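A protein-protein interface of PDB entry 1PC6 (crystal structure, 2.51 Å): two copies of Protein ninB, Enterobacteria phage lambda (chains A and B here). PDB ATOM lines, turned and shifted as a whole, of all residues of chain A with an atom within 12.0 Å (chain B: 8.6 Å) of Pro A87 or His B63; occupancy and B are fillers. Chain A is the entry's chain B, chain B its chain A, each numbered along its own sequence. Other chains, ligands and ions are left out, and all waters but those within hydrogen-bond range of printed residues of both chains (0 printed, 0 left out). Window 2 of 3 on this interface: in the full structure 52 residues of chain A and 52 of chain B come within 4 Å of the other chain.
The indole nitrogen (NE1) of Trp B62 is in hydrogen-bond range of the backbone carbonyl oxygen (O) of Pro A87 (2.7 Å).
The side-chain carboxylate (OD2) of Asp A84 lies within salt-bridge range of the guanidinium group (NH2) of Arg B65.
The side-chain amide oxygen (OD1) of Asn A88 is in hydrogen-bond range of the backbone NH (N) of Gly A93 (2.7 Å).
The backbone NH (N) of Asp A84 lies within hydrogen-bond range of the backbone carbonyl oxygen (O) of Ile A97 (2.7 Å).
O of Val A86 is in hydrogen-bond range of N of Val A95 (2.9 Å).
OD1 of Asn A88 sits at hydrogen-bond distance from N of Gly A91.
OD1 of Asn A88 is in hydrogen-bond range of N of Asn A92, 3.0 Å away.
Among the printed residues, pairs that only touch across the chains: Val A86 with Trp B62 (3.9 Å), Val A86 with Arg B65 (3.7 Å), Val A86 with Val B75 (3.9 Å), Pro A87 with His B63 (3.7 Å), Asn A88 with Trp B62 (3.5 Å), Leu A89 with Trp B62 (3.5 Å), Leu A89 with Val B75 (3.8 Å), Leu A89 with Phe B76 (3.6 Å), Leu A89 with Phe B119 (3.5 Å), Val A95 with Ala B78 (3.9 Å), Val A96 with Cys B74 (3.999 Å), Ile A97 with Ser B71 (3.8 Å) and Ile A97 with Cys B74 (3.95 Å).
Of the printed residues of chain B, Asp A84 touches Arg B65.
Pro A87 touches just these residues of chain B: Trp B62 (2.7 Å) and His B63 (3.7 Å).
Of the printed residues of chain B, Asn A88 touches Trp B62 (3.5 Å).
Phe A94 touches none of the printed residues of chain B.
Val B60 touches none of the printed residues of chain A.
No residue of chain A comes within 4 Å of Glu B61.
Trp B62 touches four residues of chain A.
His B63 touches one residue of chain A.
No residue of chain A comes within 4 Å of Gly B64.
Of the printed residues of chain A, Arg B65 touches Asp A84 (2.9 Å) and Val A86 (3.7 Å).
Of the printed residues of chain A, Cys B74 touches Val A96 (3.999 Å) and Ile A97 (3.95 Å).
Of chain A, only Val A86 and Leu A89 come within 4 Å of Val B75.
The nearest residue of chain B that does not touch Pro A87 is Val B75 (4.2 Å).
The nearest printed residue of chain B that does not touch Val A95 is Val B75 (4.1 Å).
Printed residues of chain B that touch a printed residue of chain A: Trp B62, His B63, Arg B65, Ser B71, Cys B74, Val B75, Phe B76, Ala B78 and Phe B119.
Hydrophobic or aromatic side chains of chain B that line the printed part of chain A: Trp B62, His B63, Val B75, Phe B76, Ala B78 and Phe B119.
Along chain B the printed residues that touch a printed residue of chain A span positions 62 to 119.
Among the printed residues, Asp or Glu carboxylates within 4 Å of a Lys or Arg side-chain nitrogen of the other chain: Asp A84 with Arg B65.
No position is printed for both chains.
Of the 15 pairs that touch across the chains among the printed residues, none has its exchanged pair printed and touching as well.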
ATOM      1  N   GLN A  83      39.164  13.431   5.795  1.00  0.00           N
ATOM      2  CA  GLN A  83      38.057  12.528   6.036  1.00  0.00           C
ATOM      3  C   GLN A  83      38.097  11.398   5.028  1.00  0.00           C
ATOM      4  O   GLN A  83      38.722  11.507   3.991  1.00  0.00           O
ATOM      5  CB  GLN A  83      36.736  13.311   5.912  1.00  0.00           C
ATOM      6  CG  GLN A  83      36.626  14.482   6.897  1.00  0.00           C
ATOM      7  CD  GLN A  83      35.405  15.366   6.667  1.00  0.00           C
ATOM      8  OE1 GLN A  83      35.361  16.155   5.719  1.00  0.00           O
ATOM      9  NE2 GLN A  83      34.409  15.238   7.540  1.00  0.00           N
ATOM     10  N   ASP A  84      37.436  10.304   5.339  1.00  0.00           N
ATOM     11  CA  ASP A  84      37.394   9.193   4.418  1.00  0.00           C
ATOM     12  C   ASP A  84      36.104   9.216   3.639  1.00  0.00           C
ATOM     13  O   ASP A  84      35.156   9.871   4.039  1.00  0.00           O
ATOM     14  CB  ASP A  84      37.494   7.888   5.175  1.00  0.00           C
ATOM     15  CG  ASP A  84      38.903   7.479   5.384  1.00  0.00           C
ATOM     16  OD1 ASP A  84      39.655   8.279   5.978  1.00  0.00           O
ATOM     17  OD2 ASP A  84      39.261   6.366   4.941  1.00  0.00           O
ATOM     18  N   VAL A  85      36.066   8.495   2.526  1.00  0.00           N
ATOM     19  CA  VAL A  85      34.862   8.443   1.724  1.00  0.00           C
ATOM     20  C   VAL A  85      34.603   7.017   1.259  1.00  0.00           C
ATOM     21  O   VAL A  85      35.456   6.404   0.611  1.00  0.00           O
ATOM     22  CB  VAL A  85      34.957   9.393   0.488  1.00  0.00           C
ATOM     23  CG1 VAL A  85      33.770   9.188  -0.437  1.00  0.00           C
ATOM     24  CG2 VAL A  85      34.980  10.839   0.945  1.00  0.00           C
ATOM     25  N   VAL A  86      33.429   6.495   1.622  1.00  0.00           N
ATOM     26  CA  VAL A  86      32.985   5.157   1.235  1.00  0.00           C
ATOM     27  C   VAL A  86      31.632   5.340   0.533  1.00  0.00           C
ATOM     28  O   VAL A  86      30.969   6.366   0.702  1.00  0.00           O
ATOM     29  CB  VAL A  86      32.793   4.223   2.462  1.00  0.00           C
ATOM     30  CG1 VAL A  86      34.074   4.125   3.264  1.00  0.00           C
ATOM     31  CG2 VAL A  86      31.683   4.736   3.329  1.00  0.00           C
ATOM     32  N   PRO A  87      31.204   4.351  -0.269  1.00  0.00           N
ATOM     33  CA  PRO A  87      29.922   4.448  -0.980  1.00  0.00           C
ATOM     34  C   PRO A  87      28.738   4.504  -0.029  1.00  0.00           C
ATOM     35  O   PRO A  87      28.789   3.959   1.078  1.00  0.00           O
ATOM     36  CB  PRO A  87      29.902   3.186  -1.827  1.00  0.00           C
ATOM     37  CG  PRO A  87      31.372   2.864  -2.008  1.00  0.00           C
ATOM     38  CD  PRO A  87      31.924   3.123  -0.653  1.00  0.00           C
ATOM     39  N   ASN A  88      27.672   5.168  -0.456  1.00  0.00           N
ATOM     40  CA  ASN A  88      26.474   5.267   0.373  1.00  0.00           C
ATOM     41  C   ASN A  88      25.724   3.950   0.171  1.00  0.00           C
ATOM     42  O   ASN A  88      25.970   3.243  -0.814  1.00  0.00           O
ATOM     43  CB  ASN A  88      25.618   6.459  -0.073  1.00  0.00           C
ATOM     44  CG  ASN A  88      25.030   6.259  -1.450  1.00  0.00           C
ATOM     45  OD1 ASN A  88      25.679   5.693  -2.330  1.00  0.00           O
ATOM     46  ND2 ASN A  88      23.803   6.719  -1.647  1.00  0.00           N
ATOM     47  N   LEU A  89      24.823   3.616   1.094  1.00  0.00           N
ATOM     48  CA  LEU A  89      24.073   2.359   1.006  1.00  0.00           C
ATOM     49  C   LEU A  89      23.341   2.143  -0.312  1.00  0.00           C
ATOM     50  O   LEU A  89      23.306   1.024  -0.840  1.00  0.00           O
ATOM     51  CB  LEU A  89      23.073   2.243   2.164  1.00  0.00           C
ATOM     52  CG  LEU A  89      23.644   1.830   3.523  1.00  0.00           C
ATOM     53  CD1 LEU A  89      22.571   1.919   4.576  1.00  0.00           C
ATOM     54  CD2 LEU A  89      24.198   0.424   3.440  1.00  0.00           C
ATOM     55  N   ALA A  90      22.755   3.211  -0.841  1.00  0.00           N
ATOM     56  CA  ALA A  90      22.023   3.131  -2.096  1.00  0.00           C
ATOM     57  C   ALA A  90      22.940   2.827  -3.284  1.00  0.00           C
ATOM     58  O   ALA A  90      22.484   2.314  -4.306  1.00  0.00           O
ATOM     59  CB  ALA A  90      21.282   4.432  -2.337  1.00  0.00           C
ATOM     60  N   GLY A  91      24.225   3.155  -3.150  1.00  0.00           N
ATOM     61  CA  GLY A  91      25.166   2.912  -4.225  1.00  0.00           C
ATOM     62  C   GLY A  91      25.037   3.921  -5.348  1.00  0.00           C
ATOM     63  O   GLY A  91      25.419   3.646  -6.481  1.00  0.00           O
ATOM     64  N   ASN A  92      24.493   5.091  -5.039  1.00  0.00           N
ATOM     65  CA  ASN A  92      24.335   6.142  -6.028  1.00  0.00           C
ATOM     66  C   ASN A  92      24.930   7.448  -5.510  1.00  0.00           C
ATOM     67  O   ASN A  92      24.630   8.520  -6.016  1.00  0.00           O
ATOM     68  CB  ASN A  92      22.864   6.345  -6.337  1.00  0.00           C
ATOM     69  CG  ASN A  92      22.087   6.776  -5.132  1.00  0.00           C
ATOM     70  OD1 ASN A  92      22.417   7.757  -4.487  1.00  0.00           O
ATOM     71  ND2 ASN A  92      21.041   6.041  -4.816  1.00  0.00           N
ATOM     72  N   GLY A  93      25.769   7.355  -4.490  1.00  0.00           N
ATOM     73  CA  GLY A  93      26.388   8.537  -3.919  1.00  0.00           C
ATOM     74  C   GLY A  93      27.517   8.102  -3.010  1.00  0.00           C
ATOM     75  O   GLY A  93      28.176   7.079  -3.250  1.00  0.00           O
ATOM     76  N   PHE A  94      27.743   8.846  -1.945  1.00  0.00           N
ATOM     77  CA  PHE A  94      28.826   8.476  -1.065  1.00  0.00           C
ATOM     78  C   PHE A  94      28.547   9.061   0.278  1.00  0.00           C
ATOM     79  O   PHE A  94      27.596   9.808   0.435  1.00  0.00           O
ATOM     80  CB  PHE A  94      30.126   9.055  -1.593  1.00  0.00           C
ATOM     81  CG  PHE A  94      30.153  10.560  -1.580  1.00  0.00           C
ATOM     82  CD1 PHE A  94      30.651  11.253  -0.480  1.00  0.00           C
ATOM     83  CD2 PHE A  94      29.614  11.286  -2.636  1.00  0.00           C
ATOM     84  CE1 PHE A  94      30.612  12.642  -0.427  1.00  0.00           C
ATOM     85  CE2 PHE A  94      29.569  12.679  -2.591  1.00  0.00           C
ATOM     86  CZ  PHE A  94      30.070  13.354  -1.478  1.00  0.00           C
ATOM     87  N   VAL A  95      29.383   8.715   1.247  1.00  0.00           N
ATOM     88  CA  VAL A  95      29.258   9.238   2.596  1.00  0.00           C
ATOM     89  C   VAL A  95      30.662   9.519   3.102  1.00  0.00           C
ATOM     90  O   VAL A  95      31.587   8.765   2.812  1.00  0.00           O
ATOM     91  CB  VAL A  95      28.526   8.247   3.554  1.00  0.00           C
ATOM     92  CG1 VAL A  95      28.392   6.877   2.915  1.00  0.00           C
ATOM     93  CG2 VAL A  95      29.271   8.148   4.871  1.00  0.00           C
ATOM     94  N   VAL A  96      30.832  10.626   3.822  1.00  0.00           N
ATOM     95  CA  VAL A  96      32.150  10.950   4.344  1.00  0.00           C
ATOM     96  C   VAL A  96      32.213  10.605   5.823  1.00  0.00           C
ATOM     97  O   VAL A  96      31.243  10.767   6.562  1.00  0.00           O
ATOM     98  CB  VAL A  96      32.571  12.457   4.103  1.00  0.00           C
ATOM     99  CG1 VAL A  96      31.771  13.050   2.975  1.00  0.00           C
ATOM    100  CG2 VAL A  96      32.463  13.263   5.366  1.00  0.00           C
ATOM    101  N   ILE A  97      33.376  10.109   6.226  1.00  0.00           N
ATOM    102  CA  ILE A  97      33.636   9.696   7.587  1.00  0.00           C
ATOM    103  C   ILE A  97      34.895  10.367   8.125  1.00  0.00           C
ATOM    104  O   ILE A  97      35.997  10.156   7.612  1.00  0.00           O
ATOM    105  CB  ILE A  97      33.839   8.195   7.631  1.00  0.00           C
ATOM    106  CG1 ILE A  97      32.618   7.509   7.025  1.00  0.00           C
ATOM    107  CG2 ILE A  97      34.103   7.756   9.057  1.00  0.00           C
ATOM    108  CD1 ILE A  97      32.870   6.088   6.613  1.00  0.00           C
ATOM    109  N   VAL B  60      30.005  -7.794   7.794  1.00  0.00           N
ATOM    110  CA  VAL B  60      29.856  -7.428   6.396  1.00  0.00           C
ATOM    111  C   VAL B  60      30.906  -6.434   5.876  1.00  0.00           C
ATOM    112  O   VAL B  60      31.175  -5.403   6.501  1.00  0.00           O
ATOM    113  CB  VAL B  60      28.410  -6.918   6.150  1.00  0.00           C
ATOM    114  CG1 VAL B  60      27.511  -7.379   7.290  1.00  0.00           C
ATOM    115  CG2 VAL B  60      28.376  -5.426   6.021  1.00  0.00           C
ATOM    116  N   GLU B  61      31.527  -6.748   4.742  1.00  0.00           N
ATOM    117  CA  GLU B  61      32.514  -5.824   4.213  1.00  0.00           C
ATOM    118  C   GLU B  61      31.890  -4.911   3.178  1.00  0.00           C
ATOM    119  O   GLU B  61      31.181  -5.359   2.278  1.00  0.00           O
ATOM    120  CB  GLU B  61      33.697  -6.556   3.601  1.00  0.00           C
ATOM    121  CG  GLU B  61      33.459  -7.120   2.233  1.00  0.00           C
ATOM    122  CD  GLU B  61      34.662  -6.909   1.340  1.00  0.00           C
ATOM    123  OE1 GLU B  61      35.799  -7.226   1.786  1.00  0.00           O
ATOM    124  OE2 GLU B  61      34.465  -6.422   0.197  1.00  0.00           O
ATOM    125  N   TRP B  62      32.167  -3.620   3.327  1.00  0.00           N
ATOM    126  CA  TRP B  62      31.641  -2.596   2.445  1.00  0.00           C
ATOM    127  C   TRP B  62      32.589  -2.253   1.313  1.00  0.00           C
ATOM    128  O   TRP B  62      33.624  -1.612   1.529  1.00  0.00           O
ATOM    129  CB  TRP B  62      31.372  -1.328   3.230  1.00  0.00           C
ATOM    130  CG  TRP B  62      30.432  -0.399   2.558  1.00  0.00           C
ATOM    131  CD1 TRP B  62      30.593   0.947   2.399  1.00  0.00           C
ATOM    132  CD2 TRP B  62      29.113  -0.701   2.090  1.00  0.00           C
ATOM    133  NE1 TRP B  62      29.447   1.507   1.876  1.00  0.00           N
ATOM    134  CE2 TRP B  62      28.524   0.516   1.677  1.00  0.00           C
ATOM    135  CE3 TRP B  62      28.368  -1.876   1.986  1.00  0.00           C
ATOM    136  CZ2 TRP B  62      27.234   0.588   1.170  1.00  0.00           C
ATOM    137  CZ3 TRP B  62      27.082  -1.802   1.483  1.00  0.00           C
ATOM    138  CH2 TRP B  62      26.529  -0.576   1.082  1.00  0.00           C
ATOM    139  N   HIS B  63      32.220  -2.679   0.109  1.00  0.00           N
ATOM    140  CA  HIS B  63      32.994  -2.388  -1.093  1.00  0.00           C
ATOM    141  C   HIS B  63      34.511  -2.465  -0.919  1.00  0.00           C
ATOM    142  O   HIS B  63      35.224  -1.470  -1.103  1.00  0.00           O
ATOM    143  CB  HIS B  63      32.618  -0.996  -1.638  1.00  0.00           C
ATOM    144  CG  HIS B  63      31.164  -0.835  -1.965  1.00  0.00           C
ATOM    145  ND1 HIS B  63      30.693  -0.787  -3.259  1.00  0.00           N
ATOM    146  CD2 HIS B  63      30.078  -0.702  -1.166  1.00  0.00           C
ATOM    147  CE1 HIS B  63      29.380  -0.631  -3.241  1.00  0.00           C
ATOM    148  NE2 HIS B  63      28.982  -0.575  -1.983  1.00  0.00           N
ATOM    149  N   GLY B  64      35.006  -3.641  -0.555  1.00  0.00           N
ATOM    150  CA  GLY B  64      36.442  -3.804  -0.420  1.00  0.00           C
ATOM    151  C   GLY B  64      37.130  -3.563   0.912  1.00  0.00           C
ATOM    152  O   GLY B  64      38.323  -3.845   1.033  1.00  0.00           O
ATOM    153  N   ARG B  65      36.427  -3.036   1.905  1.00  0.00           N
ATOM    154  CA  ARG B  65      37.077  -2.821   3.191  1.00  0.00           C
ATOM    155  C   ARG B  65      36.152  -2.933   4.396  1.00  0.00           C
ATOM    156  O   ARG B  65      34.943  -2.737   4.297  1.00  0.00           O
ATOM    157  CB  ARG B  65      37.814  -1.472   3.206  1.00  0.00           C
ATOM    158  CG  ARG B  65      36.949  -0.224   3.335  1.00  0.00           C
ATOM    159  CD  ARG B  65      37.848   1.013   3.363  1.00  0.00           C
ATOM    160  NE  ARG B  65      37.269   2.123   4.122  1.00  0.00           N
ATOM    161  CZ  ARG B  65      37.868   3.298   4.322  1.00  0.00           C
ATOM    162  NH1 ARG B  65      39.074   3.524   3.812  1.00  0.00           N
ATOM    163  NH2 ARG B  65      37.266   4.247   5.040  1.00  0.00           N
ATOM    164  N   TRP B  66      36.735  -3.265   5.538  1.00  0.00           N
ATOM    165  CA  TRP B  66      35.962  -3.396   6.748  1.00  0.00           C
ATOM    166  C   TRP B  66      35.922  -2.088   7.502  1.00  0.00           C
ATOM    167  O   TRP B  66      36.940  -1.432   7.693  1.00  0.00           O
ATOM    168  CB  TRP B  66      36.551  -4.494   7.617  1.00  0.00           C
ATOM    169  CG  TRP B  66      36.596  -5.804   6.903  1.00  0.00           C
ATOM    170  CD1 TRP B  66      37.517  -6.198   5.986  1.00  0.00           C
ATOM    171  CD2 TRP B  66      35.650  -6.879   7.012  1.00  0.00           C
ATOM    172  NE1 TRP B  66      37.210  -7.451   5.513  1.00  0.00           N
ATOM    173  CE2 TRP B  66      36.068  -7.892   6.128  1.00  0.00           C
ATOM    174  CE3 TRP B  66      34.491  -7.083   7.769  1.00  0.00           C
ATOM    175  CZ2 TRP B  66      35.363  -9.098   5.979  1.00  0.00           C
ATOM    176  CZ3 TRP B  66      33.792  -8.282   7.618  1.00  0.00           C
ATOM    177  CH2 TRP B  66      34.233  -9.269   6.732  1.00  0.00           C
ATOM    178  N   LEU B  67      34.729  -1.703   7.923  1.00  0.00           N
ATOM    179  CA  LEU B  67      34.555  -0.461   8.646  1.00  0.00           C
ATOM    180  C   LEU B  67      34.235  -0.746  10.095  1.00  0.00           C
ATOM    181  O   LEU B  67      33.616  -1.761  10.413  1.00  0.00           O
ATOM    182  CB  LEU B  67      33.417   0.334   8.033  1.00  0.00           C
ATOM    183  CG  LEU B  67      33.485   0.425   6.523  1.00  0.00           C
ATOM    184  CD1 LEU B  67      32.302   1.240   6.043  1.00  0.00           C
ATOM    185  CD2 LEU B  67      34.811   1.044   6.100  1.00  0.00           C
ATOM    186  N   SER B  71      32.263   4.223  11.876  1.00  0.00           N
ATOM    187  CA  SER B  71      32.161   4.440  10.449  1.00  0.00           C
ATOM    188  C   SER B  71      30.819   3.935   9.931  1.00  0.00           C
ATOM    189  O   SER B  71      30.226   4.562   9.057  1.00  0.00           O
ATOM    190  CB  SER B  71      33.309   3.729   9.724  1.00  0.00           C
ATOM    191  OG  SER B  71      34.581   4.187  10.164  1.00  0.00           O
ATOM    192  N   TRP B  72      30.334   2.808  10.453  1.00  0.00           N
ATOM    193  CA  TRP B  72      29.047   2.276  10.009  1.00  0.00           C
ATOM    194  C   TRP B  72      27.885   3.149  10.482  1.00  0.00           C
ATOM    195  O   TRP B  72      26.837   3.201   9.828  1.00  0.00           O
ATOM    196  CB  TRP B  72      28.839   0.837  10.490  1.00  0.00           C
ATOM    197  CG  TRP B  72      29.366  -0.226   9.555  1.00  0.00           C
ATOM    198  CD1 TRP B  72      30.460  -1.024   9.750  1.00  0.00           C
ATOM    199  CD2 TRP B  72      28.819  -0.607   8.284  1.00  0.00           C
ATOM    200  NE1 TRP B  72      30.625  -1.875   8.685  1.00  0.00           N
ATOM    201  CE2 TRP B  72      29.630  -1.640   7.772  1.00  0.00           C
ATOM    202  CE3 TRP B  72      27.723  -0.176   7.530  1.00  0.00           C
ATOM    203  CZ2 TRP B  72      29.376  -2.249   6.536  1.00  0.00           C
ATOM    204  CZ3 TRP B  72      27.472  -0.781   6.305  1.00  0.00           C
ATOM    205  CH2 TRP B  72      28.295  -1.807   5.821  1.00  0.00           C
ATOM    206  N   CYS B  74      27.881   6.338  10.553  1.00  0.00           N
ATOM    207  CA  CYS B  74      27.840   7.386   9.534  1.00  0.00           C
ATOM    208  C   CYS B  74      27.049   6.944   8.307  1.00  0.00           C
ATOM    209  O   CYS B  74      26.080   7.592   7.907  1.00  0.00           O
ATOM    210  CB  CYS B  74      29.258   7.755   9.089  1.00  0.00           C
ATOM    211  SG  CYS B  74      30.008   9.105   9.983  1.00  0.00           S
ATOM    212  N   VAL B  75      27.490   5.843   7.710  1.00  0.00           N
ATOM    213  CA  VAL B  75      26.851   5.302   6.527  1.00  0.00           C
ATOM    214  C   VAL B  75      25.360   5.138   6.772  1.00  0.00           C
ATOM    215  O   VAL B  75      24.529   5.569   5.967  1.00  0.00           O
ATOM    216  CB  VAL B  75      27.450   3.931   6.150  1.00  0.00           C
ATOM    217  CG1 VAL B  75      26.865   3.453   4.832  1.00  0.00           C
ATOM    218  CG2 VAL B  75      28.963   4.024   6.066  1.00  0.00           C
ATOM    219  N   PHE B  76      25.015   4.514   7.889  1.00  0.00           N
ATOM    220  CA  PHE B  76      23.616   4.310   8.185  1.00  0.00           C
ATOM    221  C   PHE B  76      22.915   5.632   8.393  1.00  0.00           C
ATOM    222  O   PHE B  76      21.864   5.861   7.816  1.00  0.00           O
ATOM    223  CB  PHE B  76      23.442   3.395   9.397  1.00  0.00           C
ATOM    224  CG  PHE B  76      23.620   1.940   9.075  1.00  0.00           C
ATOM    225  CD1 PHE B  76      22.804   1.322   8.137  1.00  0.00           C
ATOM    226  CD2 PHE B  76      24.622   1.192   9.688  1.00  0.00           C
ATOM    227  CE1 PHE B  76      22.984  -0.026   7.805  1.00  0.00           C
ATOM    228  CE2 PHE B  76      24.813  -0.159   9.366  1.00  0.00           C
ATOM    229  CZ  PHE B  76      23.993  -0.768   8.422  1.00  0.00           C
ATOM    230  N   ALA B  78      23.770   8.421   7.254  1.00  0.00           N
ATOM    231  CA  ALA B  78      23.789   9.105   5.968  1.00  0.00           C
ATOM    232  C   ALA B  78      22.602   8.693   5.117  1.00  0.00           C
ATOM    233  O   ALA B  78      22.117   9.473   4.308  1.00  0.00           O
ATOM    234  CB  ALA B  78      25.078   8.797   5.234  1.00  0.00           C
ATOM    235  N   PHE B 119      19.188  -3.940   7.279  1.00  0.00           N
ATOM    236  CA  PHE B 119      20.386  -4.101   6.474  1.00  0.00           C
ATOM    237  C   PHE B 119      21.123  -5.380   6.845  1.00  0.00           C
ATOM    238  O   PHE B 119      21.447  -6.187   5.984  1.00  0.00           O
ATOM    239  CB  PHE B 119      21.331  -2.922   6.680  1.00  0.00           C
ATOM    240  CG  PHE B 119      22.650  -3.098   6.001  1.00  0.00           C
ATOM    241  CD1 PHE B 119      22.787  -2.850   4.649  1.00  0.00           C
ATOM    242  CD2 PHE B 119      23.745  -3.559   6.702  1.00  0.00           C
ATOM    243  CE1 PHE B 119      24.008  -3.060   4.004  1.00  0.00           C
ATOM    244  CE2 PHE B 119      24.959  -3.772   6.067  1.00  0.00           C
ATOM    245  CZ  PHE B 119      25.092  -3.522   4.715  1.00  0.00           C
ATOM    246  N   ARG B 123      21.703  -9.492   5.047  1.00  0.00           N
ATOM    247  CA  ARG B 123      23.122  -9.802   4.837  1.00  0.00           C
ATOM    248  C   ARG B 123      23.525 -11.085   5.562  1.00  0.00           C
ATOM    249  O   ARG B 123      24.678 -11.508   5.480  1.00  0.00           O
ATOM    250  CB  ARG B 123      24.027  -8.654   5.319  1.00  0.00           C
ATOM    251  CG  ARG B 123      23.799  -7.313   4.644  1.00  0.00           C
ATOM    252  CD  ARG B 123      24.007  -7.405   3.162  1.00  0.00           C
ATOM    253  NE  ARG B 123      23.247  -6.374   2.470  1.00  0.00           N
ATOM    254  CZ  ARG B 123      23.788  -5.341   1.838  1.00  0.00           C
ATOM    255  NH1 ARG B 123      25.108  -5.196   1.806  1.00  0.00           N
ATOM    256  NH2 ARG B 123      23.005  -4.452   1.236  1.00  0.00           N
